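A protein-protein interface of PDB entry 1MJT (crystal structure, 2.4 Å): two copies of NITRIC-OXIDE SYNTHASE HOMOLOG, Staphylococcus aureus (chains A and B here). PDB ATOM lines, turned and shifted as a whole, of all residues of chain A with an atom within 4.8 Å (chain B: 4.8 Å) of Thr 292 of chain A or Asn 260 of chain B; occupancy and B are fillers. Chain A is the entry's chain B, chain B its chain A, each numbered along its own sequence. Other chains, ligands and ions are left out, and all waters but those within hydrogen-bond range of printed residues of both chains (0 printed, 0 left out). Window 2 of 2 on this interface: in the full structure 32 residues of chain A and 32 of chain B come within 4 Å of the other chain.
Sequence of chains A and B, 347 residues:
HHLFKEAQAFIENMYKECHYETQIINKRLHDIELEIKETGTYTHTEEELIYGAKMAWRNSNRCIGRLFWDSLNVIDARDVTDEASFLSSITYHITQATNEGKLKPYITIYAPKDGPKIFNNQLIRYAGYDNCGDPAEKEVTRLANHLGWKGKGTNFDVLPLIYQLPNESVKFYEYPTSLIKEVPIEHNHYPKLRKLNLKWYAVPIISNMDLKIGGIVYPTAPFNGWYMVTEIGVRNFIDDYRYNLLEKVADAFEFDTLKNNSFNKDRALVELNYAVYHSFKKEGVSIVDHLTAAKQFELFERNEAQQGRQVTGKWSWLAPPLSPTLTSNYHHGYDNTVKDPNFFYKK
The side-chain hydroxyl of Thr 292 of chain A sits at hydrogen-bond distance from the side-chain amide nitrogen of Asn 260 of chain B. The side-chain amide nitrogen of Asn 261 of chain B sits at hydrogen-bond distance from the side-chain carboxylate of Asp 289 of chain A (3.5 Å).
No position is printed for both chains.
OD1 of Asn 260 of chain B lies within hydrogen-bond range of NZ of Lys 265 of chain B, 3.0 Å away. The backbone NH (N) of Leu 291 of chain A sits at hydrogen-bond distance from the side-chain carboxylate (OD1) of Asp 289 of chain A, 3.1 Å away. The side-chain hydroxyl of Thr 292 of chain A is in hydrogen-bond range of the side-chain carboxylate of Asp 289 of chain A (2.5 Å).
Hydrophobic or aromatic side chains of chain B within 4 Å of the printed part of chain A: Phe 263. Of the 9 printed residues of chain A, 4 touch a printed residue of chain B. Along chain A the printed residues that touch a printed residue of chain B span positions 289 to 292. Among the printed residues, no Asp or Glu carboxylate lies within 4 Å of a Lys or Arg side-chain nitrogen of the other chain.
Thr 292 of chain A touches just one residue of chain B: Asn 260 (3.2 Å). Of chain A, only Asp 289 (3.3 Å), Leu 291 (3.7 Å) and Thr 292 (3.2 Å) come within 4 Å of Asn 260 of chain B. Of the printed residues of chain B, His 290 of chain A touches Phe 263. Of the printed residues of chain A, Lys 265 of chain B touches Leu 291. Of the printed residues of chain A, Phe 263 of chain B touches His 290 (3.9 Å). Of the printed residues of chain B, Asp 289 of chain A touches Asn 260 and Asn 261. Leu 258 of chain B touches none of the printed residues of chain A. Gln 296 of chain A touches none of the printed residues of chain B. The nearest printed residue of chain A that does not touch Phe 263 of chain B is Asp 289 of chain A (4.1 Å).
Among the printed residues, merely in contact across the chains: Asp 289 of chain A with Asn 260 of chain B (3.3 Å), His 290 of chain A with Phe 263 of chain B (3.9 Å), Leu 291 of chain A with Asn 260 of chain B (3.7 Å) and Leu 291 of chain A with Lys 265 of chain B (3.8 Å).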
ATOM      1  N   VAL A 288     -10.473  -7.812 -25.138  1.00  0.00           N
ATOM      2  CA  VAL A 288      -9.842  -8.654 -24.136  1.00  0.00           C
ATOM      3  C   VAL A 288      -9.762 -10.074 -24.687  1.00  0.00           C
ATOM      4  O   VAL A 288     -10.665 -10.529 -25.395  1.00  0.00           O
ATOM      5  CB  VAL A 288     -10.655  -8.626 -22.796  1.00  0.00           C
ATOM      6  CG1 VAL A 288     -12.032  -9.240 -22.999  1.00  0.00           C
ATOM      7  CG2 VAL A 288      -9.882  -9.333 -21.685  1.00  0.00           C
ATOM      8  N   ASP A 289      -8.668 -10.766 -24.400  1.00  0.00           N
ATOM      9  CA  ASP A 289      -8.531 -12.134 -24.870  1.00  0.00           C
ATOM     10  C   ASP A 289      -9.316 -13.052 -23.937  1.00  0.00           C
ATOM     11  O   ASP A 289      -9.622 -12.696 -22.802  1.00  0.00           O
ATOM     12  CB  ASP A 289      -7.051 -12.542 -24.946  1.00  0.00           C
ATOM     13  CG  ASP A 289      -6.378 -12.565 -23.597  1.00  0.00           C
ATOM     14  OD1 ASP A 289      -6.572 -13.553 -22.855  1.00  0.00           O
ATOM     15  OD2 ASP A 289      -5.658 -11.592 -23.281  1.00  0.00           O
ATOM     16  N   HIS A 290      -9.659 -14.227 -24.440  1.00  0.00           N
ATOM     17  CA  HIS A 290     -10.431 -15.204 -23.689  1.00  0.00           C
ATOM     18  C   HIS A 290      -9.855 -15.573 -22.320  1.00  0.00           C
ATOM     19  O   HIS A 290     -10.587 -15.639 -21.333  1.00  0.00           O
ATOM     20  CB  HIS A 290     -10.584 -16.466 -24.530  1.00  0.00           C
ATOM     21  CG  HIS A 290      -9.283 -17.014 -25.013  1.00  0.00           C
ATOM     22  ND1 HIS A 290      -8.935 -18.338 -24.870  1.00  0.00           N
ATOM     23  CD2 HIS A 290      -8.233 -16.411 -25.619  1.00  0.00           C
ATOM     24  CE1 HIS A 290      -7.725 -18.527 -25.364  1.00  0.00           C
ATOM     25  NE2 HIS A 290      -7.277 -17.374 -25.824  1.00  0.00           N
ATOM     26  N   LEU A 291      -8.552 -15.820 -22.260  1.00  0.00           N
ATOM     27  CA  LEU A 291      -7.914 -16.204 -21.009  1.00  0.00           C
ATOM     28  C   LEU A 291      -7.878 -15.073 -19.987  1.00  0.00           C
ATOM     29  O   LEU A 291      -8.065 -15.296 -18.791  1.00  0.00           O
ATOM     30  CB  LEU A 291      -6.495 -16.709 -21.280  1.00  0.00           C
ATOM     31  CG  LEU A 291      -6.410 -17.937 -22.186  1.00  0.00           C
ATOM     32  CD1 LEU A 291      -4.994 -18.499 -22.113  1.00  0.00           C
ATOM     33  CD2 LEU A 291      -7.455 -18.990 -21.758  1.00  0.00           C
ATOM     34  N   THR A 292      -7.629 -13.859 -20.459  1.00  0.00           N
ATOM     35  CA  THR A 292      -7.587 -12.699 -19.583  1.00  0.00           C
ATOM     36  C   THR A 292      -8.987 -12.419 -19.043  1.00  0.00           C
ATOM     37  O   THR A 292      -9.151 -12.065 -17.881  1.00  0.00           O
ATOM     38  CB  THR A 292      -7.075 -11.466 -20.345  1.00  0.00           C
ATOM     39  OG1 THR A 292      -5.717 -11.687 -20.747  1.00  0.00           O
ATOM     40  CG2 THR A 292      -7.145 -10.235 -19.475  1.00  0.00           C
ATOM     41  N   ALA A 293      -9.994 -12.593 -19.893  1.00  0.00           N
ATOM     42  CA  ALA A 293     -11.383 -12.364 -19.506  1.00  0.00           C
ATOM     43  C   ALA A 293     -11.808 -13.333 -18.406  1.00  0.00           C
ATOM     44  O   ALA A 293     -12.568 -12.975 -17.512  1.00  0.00           O
ATOM     45  CB  ALA A 293     -12.295 -12.519 -20.720  1.00  0.00           C
ATOM     46  N   ALA A 294     -11.314 -14.563 -18.488  1.00  0.00           N
ATOM     47  CA  ALA A 294     -11.622 -15.589 -17.498  1.00  0.00           C
ATOM     48  C   ALA A 294     -10.910 -15.303 -16.180  1.00  0.00           C
ATOM     49  O   ALA A 294     -11.396 -15.686 -15.116  1.00  0.00           O
ATOM     50  CB  ALA A 294     -11.217 -16.962 -18.018  1.00  0.00           C
ATOM     51  N   LYS A 295      -9.760 -14.637 -16.244  1.00  0.00           N
ATOM     52  CA  LYS A 295      -9.015 -14.318 -15.033  1.00  0.00           C
ATOM     53  C   LYS A 295      -9.749 -13.217 -14.293  1.00  0.00           C
ATOM     54  O   LYS A 295      -9.784 -13.195 -13.059  1.00  0.00           O
ATOM     55  CB  LYS A 295      -7.601 -13.848 -15.361  1.00  0.00           C
ATOM     56  CG  LYS A 295      -6.622 -14.024 -14.205  1.00  0.00           C
ATOM     57  CD  LYS A 295      -6.393 -15.503 -13.912  1.00  0.00           C
ATOM     58  CE  LYS A 295      -5.383 -15.716 -12.793  1.00  0.00           C
ATOM     59  NZ  LYS A 295      -5.099 -17.169 -12.581  1.00  0.00           N
ATOM     60  N   GLN A 296     -10.331 -12.300 -15.059  1.00  0.00           N
ATOM     61  CA  GLN A 296     -11.082 -11.197 -14.484  1.00  0.00           C
ATOM     62  C   GLN A 296     -12.342 -11.738 -13.820  1.00  0.00           C
ATOM     63  O   GLN A 296     -12.826 -11.187 -12.831  1.00  0.00           O
ATOM     64  CB  GLN A 296     -11.452 -10.195 -15.574  1.00  0.00           C
ATOM     65  CG  GLN A 296     -10.255  -9.469 -16.167  1.00  0.00           C
ATOM     66  CD  GLN A 296     -10.602  -8.664 -17.409  1.00  0.00           C
ATOM     67  OE1 GLN A 296     -11.658  -8.859 -18.020  1.00  0.00           O
ATOM     68  NE2 GLN A 296      -9.701  -7.767 -17.800  1.00  0.00           N
ATOM     69  N   LEU B 258       4.548 -16.399 -22.573  1.00  0.00           N
ATOM     70  CA  LEU B 258       3.266 -17.069 -22.448  1.00  0.00           C
ATOM     71  C   LEU B 258       2.158 -16.076 -22.060  1.00  0.00           C
ATOM     72  O   LEU B 258       1.066 -16.485 -21.642  1.00  0.00           O
ATOM     73  CB  LEU B 258       3.345 -18.203 -21.418  1.00  0.00           C
ATOM     74  CG  LEU B 258       4.008 -19.505 -21.862  1.00  0.00           C
ATOM     75  CD1 LEU B 258       3.994 -20.481 -20.702  1.00  0.00           C
ATOM     76  CD2 LEU B 258       3.275 -20.097 -23.058  1.00  0.00           C
ATOM     77  N   LYS B 259       2.433 -14.777 -22.191  1.00  0.00           N
ATOM     78  CA  LYS B 259       1.424 -13.785 -21.864  1.00  0.00           C
ATOM     79  C   LYS B 259       0.175 -14.123 -22.660  1.00  0.00           C
ATOM     80  O   LYS B 259       0.272 -14.526 -23.819  1.00  0.00           O
ATOM     81  CB  LYS B 259       1.913 -12.381 -22.204  1.00  0.00           C
ATOM     82  CG  LYS B 259       3.007 -11.909 -21.262  1.00  0.00           C
ATOM     83  CD  LYS B 259       3.222 -10.402 -21.322  1.00  0.00           C
ATOM     84  CE  LYS B 259       4.216  -9.955 -20.249  1.00  0.00           C
ATOM     85  NZ  LYS B 259       4.399  -8.476 -20.213  1.00  0.00           N
ATOM     86  N   ASN B 260      -0.993 -13.980 -22.035  1.00  0.00           N
ATOM     87  CA  ASN B 260      -2.245 -14.293 -22.702  1.00  0.00           C
ATOM     88  C   ASN B 260      -2.366 -13.613 -24.069  1.00  0.00           C
ATOM     89  O   ASN B 260      -2.930 -14.185 -25.005  1.00  0.00           O
ATOM     90  CB  ASN B 260      -3.424 -13.921 -21.799  1.00  0.00           C
ATOM     91  CG  ASN B 260      -3.464 -14.754 -20.518  1.00  0.00           C
ATOM     92  OD1 ASN B 260      -2.867 -15.830 -20.438  1.00  0.00           O
ATOM     93  ND2 ASN B 260      -4.182 -14.264 -19.514  1.00  0.00           N
ATOM     94  N   ASN B 261      -1.815 -12.406 -24.171  1.00  0.00           N
ATOM     95  CA  ASN B 261      -1.816 -11.609 -25.403  1.00  0.00           C
ATOM     96  C   ASN B 261      -1.136 -12.282 -26.577  1.00  0.00           C
ATOM     97  O   ASN B 261      -1.507 -12.051 -27.722  1.00  0.00           O
ATOM     98  CB  ASN B 261      -1.094 -10.279 -25.177  1.00  0.00           C
ATOM     99  CG  ASN B 261      -2.031  -9.169 -24.828  1.00  0.00           C
ATOM    100  OD1 ASN B 261      -1.617  -8.028 -24.638  1.00  0.00           O
ATOM    101  ND2 ASN B 261      -3.314  -9.491 -24.738  1.00  0.00           N
ATOM    102  N   SER B 262      -0.112 -13.080 -26.281  1.00  0.00           N
ATOM    103  CA  SER B 262       0.683 -13.776 -27.293  1.00  0.00           C
ATOM    104  C   SER B 262      -0.054 -14.918 -27.961  1.00  0.00           C
ATOM    105  O   SER B 262       0.226 -15.259 -29.111  1.00  0.00           O
ATOM    106  CB  SER B 262       1.954 -14.341 -26.657  1.00  0.00           C
ATOM    107  OG  SER B 262       1.648 -15.483 -25.869  1.00  0.00           O
ATOM    108  N   PHE B 263      -0.988 -15.511 -27.227  1.00  0.00           N
ATOM    109  CA  PHE B 263      -1.757 -16.653 -27.708  1.00  0.00           C
ATOM    110  C   PHE B 263      -0.827 -17.856 -27.829  1.00  0.00           C
ATOM    111  O   PHE B 263      -1.153 -18.840 -28.483  1.00  0.00           O
ATOM    112  CB  PHE B 263      -2.425 -16.356 -29.059  1.00  0.00           C
ATOM    113  CG  PHE B 263      -3.610 -15.425 -28.962  1.00  0.00           C
ATOM    114  CD1 PHE B 263      -3.430 -14.047 -28.889  1.00  0.00           C
ATOM    115  CD2 PHE B 263      -4.904 -15.933 -28.902  1.00  0.00           C
ATOM    116  CE1 PHE B 263      -4.520 -13.181 -28.752  1.00  0.00           C
ATOM    117  CE2 PHE B 263      -6.002 -15.083 -28.766  1.00  0.00           C
ATOM    118  CZ  PHE B 263      -5.808 -13.698 -28.689  1.00  0.00           C
ATOM    119  N   LYS B 265       0.080 -19.695 -25.284  1.00  0.00           N
ATOM    120  CA  LYS B 265      -0.484 -20.734 -24.433  1.00  0.00           C
ATOM    121  C   LYS B 265      -1.377 -21.594 -25.322  1.00  0.00           C
ATOM    122  O   LYS B 265      -1.375 -22.820 -25.226  1.00  0.00           O
ATOM    123  CB  LYS B 265      -1.321 -20.132 -23.303  1.00  0.00           C
ATOM    124  CG  LYS B 265      -0.523 -19.570 -22.150  1.00  0.00           C
ATOM    125  CD  LYS B 265      -1.460 -19.229 -21.010  1.00  0.00           C
ATOM    126  CE  LYS B 265      -0.740 -18.493 -19.901  1.00  0.00           C
ATOM    127  NZ  LYS B 265      -1.689 -18.056 -18.833  1.00  0.00           N
